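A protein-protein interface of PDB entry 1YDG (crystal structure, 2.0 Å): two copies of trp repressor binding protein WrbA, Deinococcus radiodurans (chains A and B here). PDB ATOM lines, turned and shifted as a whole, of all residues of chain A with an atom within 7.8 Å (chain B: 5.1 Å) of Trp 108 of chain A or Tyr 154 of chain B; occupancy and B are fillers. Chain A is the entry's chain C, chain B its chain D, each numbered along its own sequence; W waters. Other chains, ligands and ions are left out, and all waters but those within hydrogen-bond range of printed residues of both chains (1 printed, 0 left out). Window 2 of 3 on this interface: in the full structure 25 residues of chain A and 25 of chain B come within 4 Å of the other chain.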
ATOM      1  N   ILE A 101      35.350  12.563  18.528  1.00  0.00           N
ATOM      2  CA  ILE A 101      34.746  11.611  19.473  1.00  0.00           C
ATOM      3  C   ILE A 101      33.279  11.975  19.780  1.00  0.00           C
ATOM      4  O   ILE A 101      32.391  11.112  19.769  1.00  0.00           O
ATOM      5  CB  ILE A 101      35.616  11.546  20.759  1.00  0.00           C
ATOM      6  CG1 ILE A 101      36.835  10.654  20.499  1.00  0.00           C
ATOM      7  CG2 ILE A 101      34.826  11.089  22.003  1.00  0.00           C
ATOM      8  CD1 ILE A 101      38.003  10.895  21.487  1.00  0.00           C
ATOM      9  N   THR A 103      31.114  13.286  17.975  1.00  0.00           N
ATOM     10  CA  THR A 103      30.178  13.045  16.864  1.00  0.00           C
ATOM     11  C   THR A 103      29.797  11.553  16.731  1.00  0.00           C
ATOM     12  O   THR A 103      29.060  11.178  15.824  1.00  0.00           O
ATOM     13  CB  THR A 103      30.739  13.505  15.494  1.00  0.00           C
ATOM     14  OG1 THR A 103      31.805  12.639  15.074  1.00  0.00           O
ATOM     15  CG2 THR A 103      31.236  14.937  15.565  1.00  0.00           C
ATOM     16  N   LEU A 104      30.304  10.714  17.636  1.00  0.00           N
ATOM     17  CA  LEU A 104      30.090   9.274  17.577  1.00  0.00           C
ATOM     18  C   LEU A 104      28.884   8.809  18.389  1.00  0.00           C
ATOM     19  O   LEU A 104      28.655   7.605  18.504  1.00  0.00           O
ATOM     20  CB  LEU A 104      31.356   8.544  18.042  1.00  0.00           C
ATOM     21  CG  LEU A 104      32.619   8.900  17.262  1.00  0.00           C
ATOM     22  CD1 LEU A 104      33.819   8.144  17.844  1.00  0.00           C
ATOM     23  CD2 LEU A 104      32.472   8.608  15.756  1.00  0.00           C
ATOM     24  N   GLY A 105      28.104   9.759  18.914  1.00  0.00           N
ATOM     25  CA  GLY A 105      26.975   9.470  19.794  1.00  0.00           C
ATOM     26  C   GLY A 105      25.907   8.579  19.186  1.00  0.00           C
ATOM     27  O   GLY A 105      25.370   7.691  19.860  1.00  0.00           O
ATOM     28  N   GLY A 106      25.603   8.828  17.912  1.00  0.00           N
ATOM     29  CA  GLY A 106      24.669   8.031  17.134  1.00  0.00           C
ATOM     30  C   GLY A 106      25.078   6.590  16.932  1.00  0.00           C
ATOM     31  O   GLY A 106      24.259   5.684  17.140  1.00  0.00           O
ATOM     32  N   LEU A 107      26.332   6.361  16.525  1.00  0.00           N
ATOM     33  CA  LEU A 107      26.880   5.003  16.470  1.00  0.00           C
ATOM     34  C   LEU A 107      26.856   4.334  17.833  1.00  0.00           C
ATOM     35  O   LEU A 107      26.451   3.178  17.968  1.00  0.00           O
ATOM     36  CB  LEU A 107      28.328   4.997  15.976  1.00  0.00           C
ATOM     37  CG  LEU A 107      28.619   5.260  14.509  1.00  0.00           C
ATOM     38  CD1 LEU A 107      30.115   5.205  14.293  1.00  0.00           C
ATOM     39  CD2 LEU A 107      27.889   4.260  13.624  1.00  0.00           C
ATOM     40  N   TRP A 108      27.318   5.058  18.841  1.00  0.00           N
ATOM     41  CA  TRP A 108      27.316   4.546  20.205  1.00  0.00           C
ATOM     42  C   TRP A 108      25.903   4.118  20.649  1.00  0.00           C
ATOM     43  O   TRP A 108      25.735   3.032  21.194  1.00  0.00           O
ATOM     44  CB  TRP A 108      27.919   5.587  21.143  1.00  0.00           C
ATOM     45  CG  TRP A 108      27.840   5.253  22.583  1.00  0.00           C
ATOM     46  CD1 TRP A 108      28.546   4.290  23.251  1.00  0.00           C
ATOM     47  CD2 TRP A 108      27.011   5.893  23.556  1.00  0.00           C
ATOM     48  NE1 TRP A 108      28.196   4.287  24.584  1.00  0.00           N
ATOM     49  CE2 TRP A 108      27.261   5.262  24.799  1.00  0.00           C
ATOM     50  CE3 TRP A 108      26.084   6.944  23.502  1.00  0.00           C
ATOM     51  CZ2 TRP A 108      26.616   5.641  25.969  1.00  0.00           C
ATOM     52  CZ3 TRP A 108      25.441   7.321  24.656  1.00  0.00           C
ATOM     53  CH2 TRP A 108      25.712   6.673  25.886  1.00  0.00           C
ATOM     54  N   SER A 109      24.898   4.956  20.400  1.00  0.00           N
ATOM     55  CA  SER A 109      23.496   4.631  20.737  1.00  0.00           C
ATOM     56  C   SER A 109      22.994   3.359  20.057  1.00  0.00           C
ATOM     57  O   SER A 109      22.170   2.630  20.599  1.00  0.00           O
ATOM     58  CB  SER A 109      22.565   5.769  20.323  1.00  0.00           C
ATOM     59  OG  SER A 109      22.877   6.945  21.006  1.00  0.00           O
ATOM     60  N   SER A 110      23.501   3.101  18.865  1.00  0.00           N
ATOM     61  CA  SER A 110      23.071   1.982  18.067  1.00  0.00           C
ATOM     62  C   SER A 110      23.833   0.686  18.332  1.00  0.00           C
ATOM     63  O   SER A 110      23.636  -0.288  17.621  1.00  0.00           O
ATOM     64  CB  SER A 110      23.251   2.369  16.617  1.00  0.00           C
ATOM     65  OG  SER A 110      22.797   3.699  16.431  1.00  0.00           O
ATOM     66  N   GLY A 111      24.713   0.687  19.330  1.00  0.00           N
ATOM     67  CA  GLY A 111      25.562  -0.457  19.637  1.00  0.00           C
ATOM     68  C   GLY A 111      26.595  -0.751  18.564  1.00  0.00           C
ATOM     69  O   GLY A 111      27.183  -1.836  18.539  1.00  0.00           O
ATOM     70  N   LYS A 112      26.844   0.234  17.704  1.00  0.00           N
ATOM     71  CA  LYS A 112      27.632   0.038  16.486  1.00  0.00           C
ATOM     72  C   LYS A 112      29.127   0.359  16.598  1.00  0.00           C
ATOM     73  O   LYS A 112      29.807   0.422  15.573  1.00  0.00           O
ATOM     74  CB  LYS A 112      27.013   0.854  15.350  1.00  0.00           C
ATOM     75  CG  LYS A 112      25.809   0.177  14.721  1.00  0.00           C
ATOM     76  CD  LYS A 112      25.140   1.096  13.718  1.00  0.00           C
ATOM     77  CE  LYS A 112      24.029   0.392  12.967  1.00  0.00           C
ATOM     78  NZ  LYS A 112      23.012   1.411  12.531  1.00  0.00           N
ATOM     79  N   LEU A 113      29.629   0.550  17.819  1.00  0.00           N
ATOM     80  CA  LEU A 113      31.074   0.669  18.074  1.00  0.00           C
ATOM     81  C   LEU A 113      31.629  -0.505  18.881  1.00  0.00           C
ATOM     82  O   LEU A 113      32.854  -0.622  19.088  1.00  0.00           O
ATOM     83  CB  LEU A 113      31.356   1.959  18.821  1.00  0.00           C
ATOM     84  CG  LEU A 113      31.179   3.237  18.009  1.00  0.00           C
ATOM     85  CD1 LEU A 113      31.087   4.419  18.928  1.00  0.00           C
ATOM     86  CD2 LEU A 113      32.327   3.408  17.049  1.00  0.00           C
ATOM     87  N   ALA A 114      30.727  -1.369  19.342  1.00  0.00           N
ATOM     88  CA  ALA A 114      31.091  -2.474  20.212  1.00  0.00           C
ATOM     89  C   ALA A 114      31.896  -3.527  19.473  1.00  0.00           C
ATOM     90  O   ALA A 114      31.742  -3.708  18.266  1.00  0.00           O
ATOM     91  CB  ALA A 114      29.840  -3.111  20.808  1.00  0.00           C
ATOM     92  N   THR A 141      37.611   6.328  27.114  1.00  0.00           N
ATOM     93  CA  THR A 141      36.562   6.586  26.125  1.00  0.00           C
ATOM     94  C   THR A 141      36.158   5.334  25.341  1.00  0.00           C
ATOM     95  O   THR A 141      34.968   5.040  25.201  1.00  0.00           O
ATOM     96  CB  THR A 141      36.986   7.725  25.150  1.00  0.00           C
ATOM     97  OG1 THR A 141      36.929   8.970  25.845  1.00  0.00           O
ATOM     98  CG2 THR A 141      36.073   7.800  23.974  1.00  0.00           C
ATOM     99  N   ALA A 142      37.135   4.588  24.845  1.00  0.00           N
ATOM    100  CA  ALA A 142      36.845   3.351  24.116  1.00  0.00           C
ATOM    101  C   ALA A 142      36.101   2.280  24.950  1.00  0.00           C
ATOM    102  O   ALA A 142      35.334   1.469  24.407  1.00  0.00           O
ATOM    103  CB  ALA A 142      38.128   2.778  23.526  1.00  0.00           C
ATOM    104  N   MET A 143      36.314   2.284  26.259  1.00  0.00           N
ATOM    105  CA  MET A 143      35.567   1.389  27.172  1.00  0.00           C
ATOM    106  C   MET A 143      34.050   1.645  27.183  1.00  0.00           C
ATOM    107  O   MET A 143      33.272   0.706  27.327  1.00  0.00           O
ATOM    108  CB  MET A 143      36.083   1.527  28.606  1.00  0.00           C
ATOM    109  CG  MET A 143      37.529   1.111  28.773  1.00  0.00           C
ATOM    110  SD  MET A 143      37.907   0.772  30.476  1.00  0.00           S
ATOM    111  CE  MET A 143      39.687   0.635  30.385  1.00  0.00           C
ATOM    112  N   HIS A 144      33.654   2.911  27.051  1.00  0.00           N
ATOM    113  CA  HIS A 144      32.244   3.286  26.936  1.00  0.00           C
ATOM    114  C   HIS A 144      31.645   2.690  25.668  1.00  0.00           C
ATOM    115  O   HIS A 144      30.443   2.437  25.612  1.00  0.00           O
ATOM    116  CB  HIS A 144      32.058   4.805  26.912  1.00  0.00           C
ATOM    117  CG  HIS A 144      32.284   5.465  28.232  1.00  0.00           C
ATOM    118  ND1 HIS A 144      31.257   6.007  28.979  1.00  0.00           N
ATOM    119  CD2 HIS A 144      33.417   5.657  28.950  1.00  0.00           C
ATOM    120  CE1 HIS A 144      31.754   6.506  30.097  1.00  0.00           C
ATOM    121  NE2 HIS A 144      33.063   6.322  30.098  1.00  0.00           N
ATOM    122  N   TRP A 145      32.475   2.436  24.659  1.00  0.00           N
ATOM    123  CA  TRP A 145      31.986   1.787  23.439  1.00  0.00           C
ATOM    124  C   TRP A 145      31.877   0.276  23.526  1.00  0.00           C
ATOM    125  O   TRP A 145      31.321  -0.353  22.625  1.00  0.00           O
ATOM    126  CB  TRP A 145      32.880   2.129  22.263  1.00  0.00           C
ATOM    127  CG  TRP A 145      33.110   3.561  22.107  1.00  0.00           C
ATOM    128  CD1 TRP A 145      32.360   4.570  22.609  1.00  0.00           C
ATOM    129  CD2 TRP A 145      34.159   4.168  21.354  1.00  0.00           C
ATOM    130  NE1 TRP A 145      32.899   5.773  22.254  1.00  0.00           N
ATOM    131  CE2 TRP A 145      33.999   5.557  21.472  1.00  0.00           C
ATOM    132  CE3 TRP A 145      35.235   3.669  20.621  1.00  0.00           C
ATOM    133  CZ2 TRP A 145      34.867   6.461  20.867  1.00  0.00           C
ATOM    134  CZ3 TRP A 145      36.104   4.577  20.009  1.00  0.00           C
ATOM    135  CH2 TRP A 145      35.912   5.947  20.144  1.00  0.00           C
ATOM    136  N   GLY A 146      32.425  -0.340  24.564  1.00  0.00           N
ATOM    137  CA  GLY A 146      32.537  -1.809  24.567  1.00  0.00           C
ATOM    138  C   GLY A 146      33.571  -2.279  23.542  1.00  0.00           C
ATOM    139  O   GLY A 146      33.456  -3.354  22.966  1.00  0.00           O
ATOM    140  N   ALA A 147      34.590  -1.466  23.293  1.00  0.00           N
ATOM    141  CA  ALA A 147      35.662  -1.874  22.398  1.00  0.00           C
ATOM    142  C   ALA A 147      36.545  -2.890  23.110  1.00  0.00           C
ATOM    143  O   ALA A 147      36.494  -3.017  24.329  1.00  0.00           O
ATOM    144  CB  ALA A 147      36.483  -0.674  21.964  1.00  0.00           C
ATOM    145  N   PRO B 152      32.798  -4.158  30.083  1.00  0.00           N
ATOM    146  CA  PRO B 152      31.452  -4.369  29.540  1.00  0.00           C
ATOM    147  C   PRO B 152      30.910  -3.255  28.636  1.00  0.00           C
ATOM    148  O   PRO B 152      30.077  -3.539  27.792  1.00  0.00           O
ATOM    149  CB  PRO B 152      30.590  -4.498  30.799  1.00  0.00           C
ATOM    150  CG  PRO B 152      31.340  -3.764  31.840  1.00  0.00           C
ATOM    151  CD  PRO B 152      32.779  -3.938  31.540  1.00  0.00           C
ATOM    152  N   GLY B 153      31.337  -2.004  28.812  1.00  0.00           N
ATOM    153  CA  GLY B 153      30.676  -0.891  28.113  1.00  0.00           C
ATOM    154  C   GLY B 153      29.193  -0.821  28.464  1.00  0.00           C
ATOM    155  O   GLY B 153      28.811  -1.192  29.569  1.00  0.00           O
ATOM    156  N   TYR B 154      28.364  -0.346  27.535  1.00  0.00           N
ATOM    157  CA  TYR B 154      26.894  -0.401  27.673  1.00  0.00           C
ATOM    158  C   TYR B 154      26.304  -1.422  26.682  1.00  0.00           C
ATOM    159  O   TYR B 154      25.247  -1.203  26.083  1.00  0.00           O
ATOM    160  CB  TYR B 154      26.249   0.986  27.463  1.00  0.00           C
ATOM    161  CG  TYR B 154      26.711   2.053  28.440  1.00  0.00           C
ATOM    162  CD1 TYR B 154      27.846   2.818  28.171  1.00  0.00           C
ATOM    163  CD2 TYR B 154      26.008   2.316  29.621  1.00  0.00           C
ATOM    164  CE1 TYR B 154      28.296   3.801  29.060  1.00  0.00           C
ATOM    165  CE2 TYR B 154      26.445   3.313  30.516  1.00  0.00           C
ATOM    166  CZ  TYR B 154      27.596   4.052  30.229  1.00  0.00           C
ATOM    167  OH  TYR B 154      28.052   5.044  31.090  1.00  0.00           O
ATOM    168  N   THR B 155      26.987  -2.546  26.526  1.00  0.00           N
ATOM    169  CA  THR B 155      26.610  -3.573  25.546  1.00  0.00           C
ATOM    170  C   THR B 155      25.341  -4.387  25.938  1.00  0.00           C
ATOM    171  O   THR B 155      24.953  -5.321  25.215  1.00  0.00           O
ATOM    172  CB  THR B 155      27.827  -4.505  25.261  1.00  0.00           C
ATOM    173  OG1 THR B 155      28.286  -5.098  26.487  1.00  0.00           O
ATOM    174  CG2 THR B 155      28.976  -3.694  24.647  1.00  0.00           C
ATOM    175  N   ASP B 156      24.708  -4.025  27.063  1.00  0.00           N
ATOM    176  CA  ASP B 156      23.383  -4.537  27.432  1.00  0.00           C
ATOM    177  C   ASP B 156      22.534  -3.491  28.172  1.00  0.00           C
ATOM    178  O   ASP B 156      23.060  -2.544  28.770  1.00  0.00           O
ATOM    179  CB  ASP B 156      23.526  -5.770  28.312  1.00  0.00           C
ATOM    180  CG  ASP B 156      22.315  -6.714  28.221  1.00  0.00           C
ATOM    181  OD1 ASP B 156      22.226  -7.480  27.226  1.00  0.00           O
ATOM    182  OD2 ASP B 156      21.474  -6.706  29.149  1.00  0.00           O
ATOM    183  N   ILE B 159      23.328  -2.811  32.144  1.00  0.00           N
ATOM    184  CA  ILE B 159      24.344  -1.843  32.609  1.00  0.00           C
ATOM    185  C   ILE B 159      23.655  -0.560  33.062  1.00  0.00           C
ATOM    186  O   ILE B 159      23.826  -0.127  34.210  1.00  0.00           O
ATOM    187  CB  ILE B 159      25.421  -1.479  31.521  1.00  0.00           C
ATOM    188  CG1 ILE B 159      25.911  -2.713  30.753  1.00  0.00           C
ATOM    189  CG2 ILE B 159      26.622  -0.776  32.165  1.00  0.00           C
ATOM    190  CD1 ILE B 159      26.388  -3.837  31.630  1.00  0.00           C
ATOM    191  N   PHE B 160      22.880   0.030  32.147  1.00  0.00           N
ATOM    192  CA  PHE B 160      22.005   1.175  32.448  1.00  0.00           C
ATOM    193  C   PHE B 160      21.210   0.912  33.733  1.00  0.00           C
ATOM    194  O   PHE B 160      21.258   1.693  34.685  1.00  0.00           O
ATOM    195  CB  PHE B 160      21.007   1.434  31.296  1.00  0.00           C
ATOM    196  CG  PHE B 160      21.624   2.038  30.049  1.00  0.00           C
ATOM    197  CD1 PHE B 160      22.154   3.329  30.068  1.00  0.00           C
ATOM    198  CD2 PHE B 160      21.634   1.335  28.843  1.00  0.00           C
ATOM    199  CE1 PHE B 160      22.712   3.908  28.905  1.00  0.00           C
ATOM    200  CE2 PHE B 160      22.189   1.901  27.682  1.00  0.00           C
ATOM    201  CZ  PHE B 160      22.724   3.193  27.717  1.00  0.00           C
ATOM    202  N   GLY B 164      24.809   2.064  35.398  1.00  0.00           N
ATOM    203  CA  GLY B 164      25.621   2.239  34.192  1.00  0.00           C
ATOM    204  C   GLY B 164      27.107   2.488  34.380  1.00  0.00           C
ATOM    205  O   GLY B 164      27.567   3.627  34.163  1.00  0.00           O
ATOM    206  N   ASN B 165      27.860   1.451  34.775  1.00  0.00           N
ATOM    207  CA  ASN B 165      29.329   1.542  34.815  1.00  0.00           C
ATOM    208  C   ASN B 165      29.933   0.729  33.667  1.00  0.00           C
ATOM    209  O   ASN B 165      29.968  -0.498  33.713  1.00  0.00           O
ATOM    210  CB  ASN B 165      29.898   1.098  36.169  1.00  0.00           C
ATOM    211  CG  ASN B 165      31.388   1.499  36.356  1.00  0.00           C
ATOM    212  OD1 ASN B 165      32.207   1.423  35.415  1.00  0.00           O
ATOM    213  ND2 ASN B 165      31.742   1.882  37.587  1.00  0.00           N
ATOM    214  N   PRO B 166      30.407   1.417  32.617  1.00  0.00           N
ATOM    215  CA  PRO B 166      30.957   0.731  31.474  1.00  0.00           C
ATOM    216  C   PRO B 166      32.334   0.130  31.693  1.00  0.00           C
ATOM    217  O   PRO B 166      32.806  -0.654  30.858  1.00  0.00           O
ATOM    218  CB  PRO B 166      31.026   1.851  30.426  1.00  0.00           C
ATOM    219  CG  PRO B 166      31.279   3.044  31.206  1.00  0.00           C
ATOM    220  CD  PRO B 166      30.449   2.878  32.432  1.00  0.00           C
HETATM  221  O   HOH W   1      28.936   0.419  25.004  1.00  0.00           O
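The backbone carbonyl oxygen (O) of Trp 145 of chain A lies close to the backbone NH (N) of Ala 114 of chain A (3.5 Å). The backbone carbonyl oxygen of Gly 164 of chain B is in hydrogen-bond range of the side-chain hydroxyl of Tyr 154 of chain B. The backbone carbonyl oxygen (O) of Pro 152 of chain B is in hydrogen-bond range of the side-chain hydroxyl (OG1) of Thr 155 of chain B, at 2.7 Å. The backbone carbonyl oxygen of His 144 of chain A sits at hydrogen-bond distance from the indole nitrogen of Trp 108 of chain A, at 3.1 Å. The backbone NH (N) of Gly 153 of chain B lies within hydrogen-bond range of the backbone carbonyl oxygen (O) of Pro 166 of chain B (2.9 Å).
Tyr 154 of chain B touches Trp 108 of chain A (CD1 to CZ2, 3.8 Å). CB of Ala 114 of chain A touches CG2 of Thr 155 of chain B (3.98 Å). CA of Gly 153 of chain B touches O of Met 143 of chain A (3.1 Å). Pro 166 of chain B touches Met 143 of chain A (O to O, 3.8 Å). His 144 of chain A touches Tyr 154 of chain B. His 144 of chain A touches Pro 166 of chain B. CA of Gly 153 of chain B touches N of Gly 146 of chain A, 3.99 Å away.
Of chain B, only Tyr 154 (3.8 Å) comes within 4 Å of Trp 108 of chain A. Of the printed residues of chain B, Met 143 of chain A touches Gly 153 (3.1 Å) and Pro 166 (3.8 Å). Of the printed residues of chain A, Gly 153 of chain B touches Met 143 (3.1 Å) and Gly 146 (3.99 Å). Tyr 154 of chain B touches just these residues of chain A: Trp 108 (3.8 Å) and His 144 (3.7 Å). Ile 159 of chain B touches none of the printed residues of chain A. Of the printed residues of chain A, Pro 166 of chain B touches Met 143 (3.8 Å) and His 144 (3.7 Å). The nearest printed residue of chain A that does not touch Tyr 154 of chain B is Met 143 of chain A (5.0 Å). The nearest printed residue of chain B that does not touch Gly 146 of chain A is Thr 155 of chain B (4.03 Å).
Of the 20 printed residues of chain A, 5 touch a printed residue of chain B. Among the printed residues, 7 pairs touch across the chains. Among the printed residues, no Asp or Glu carboxylate lies within 4 Å of a Lys or Arg side-chain nitrogen of the other chain.
No position is printed for both chains. Of the 7 pairs that touch across the chains among the printed residues, none has its exchanged pair printed and touching as well.
Water W1 lies within hydrogen-bond range of O of His 144 of chain A, N of Tyr 154 of chain B and O of Trp 145 of chain A.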
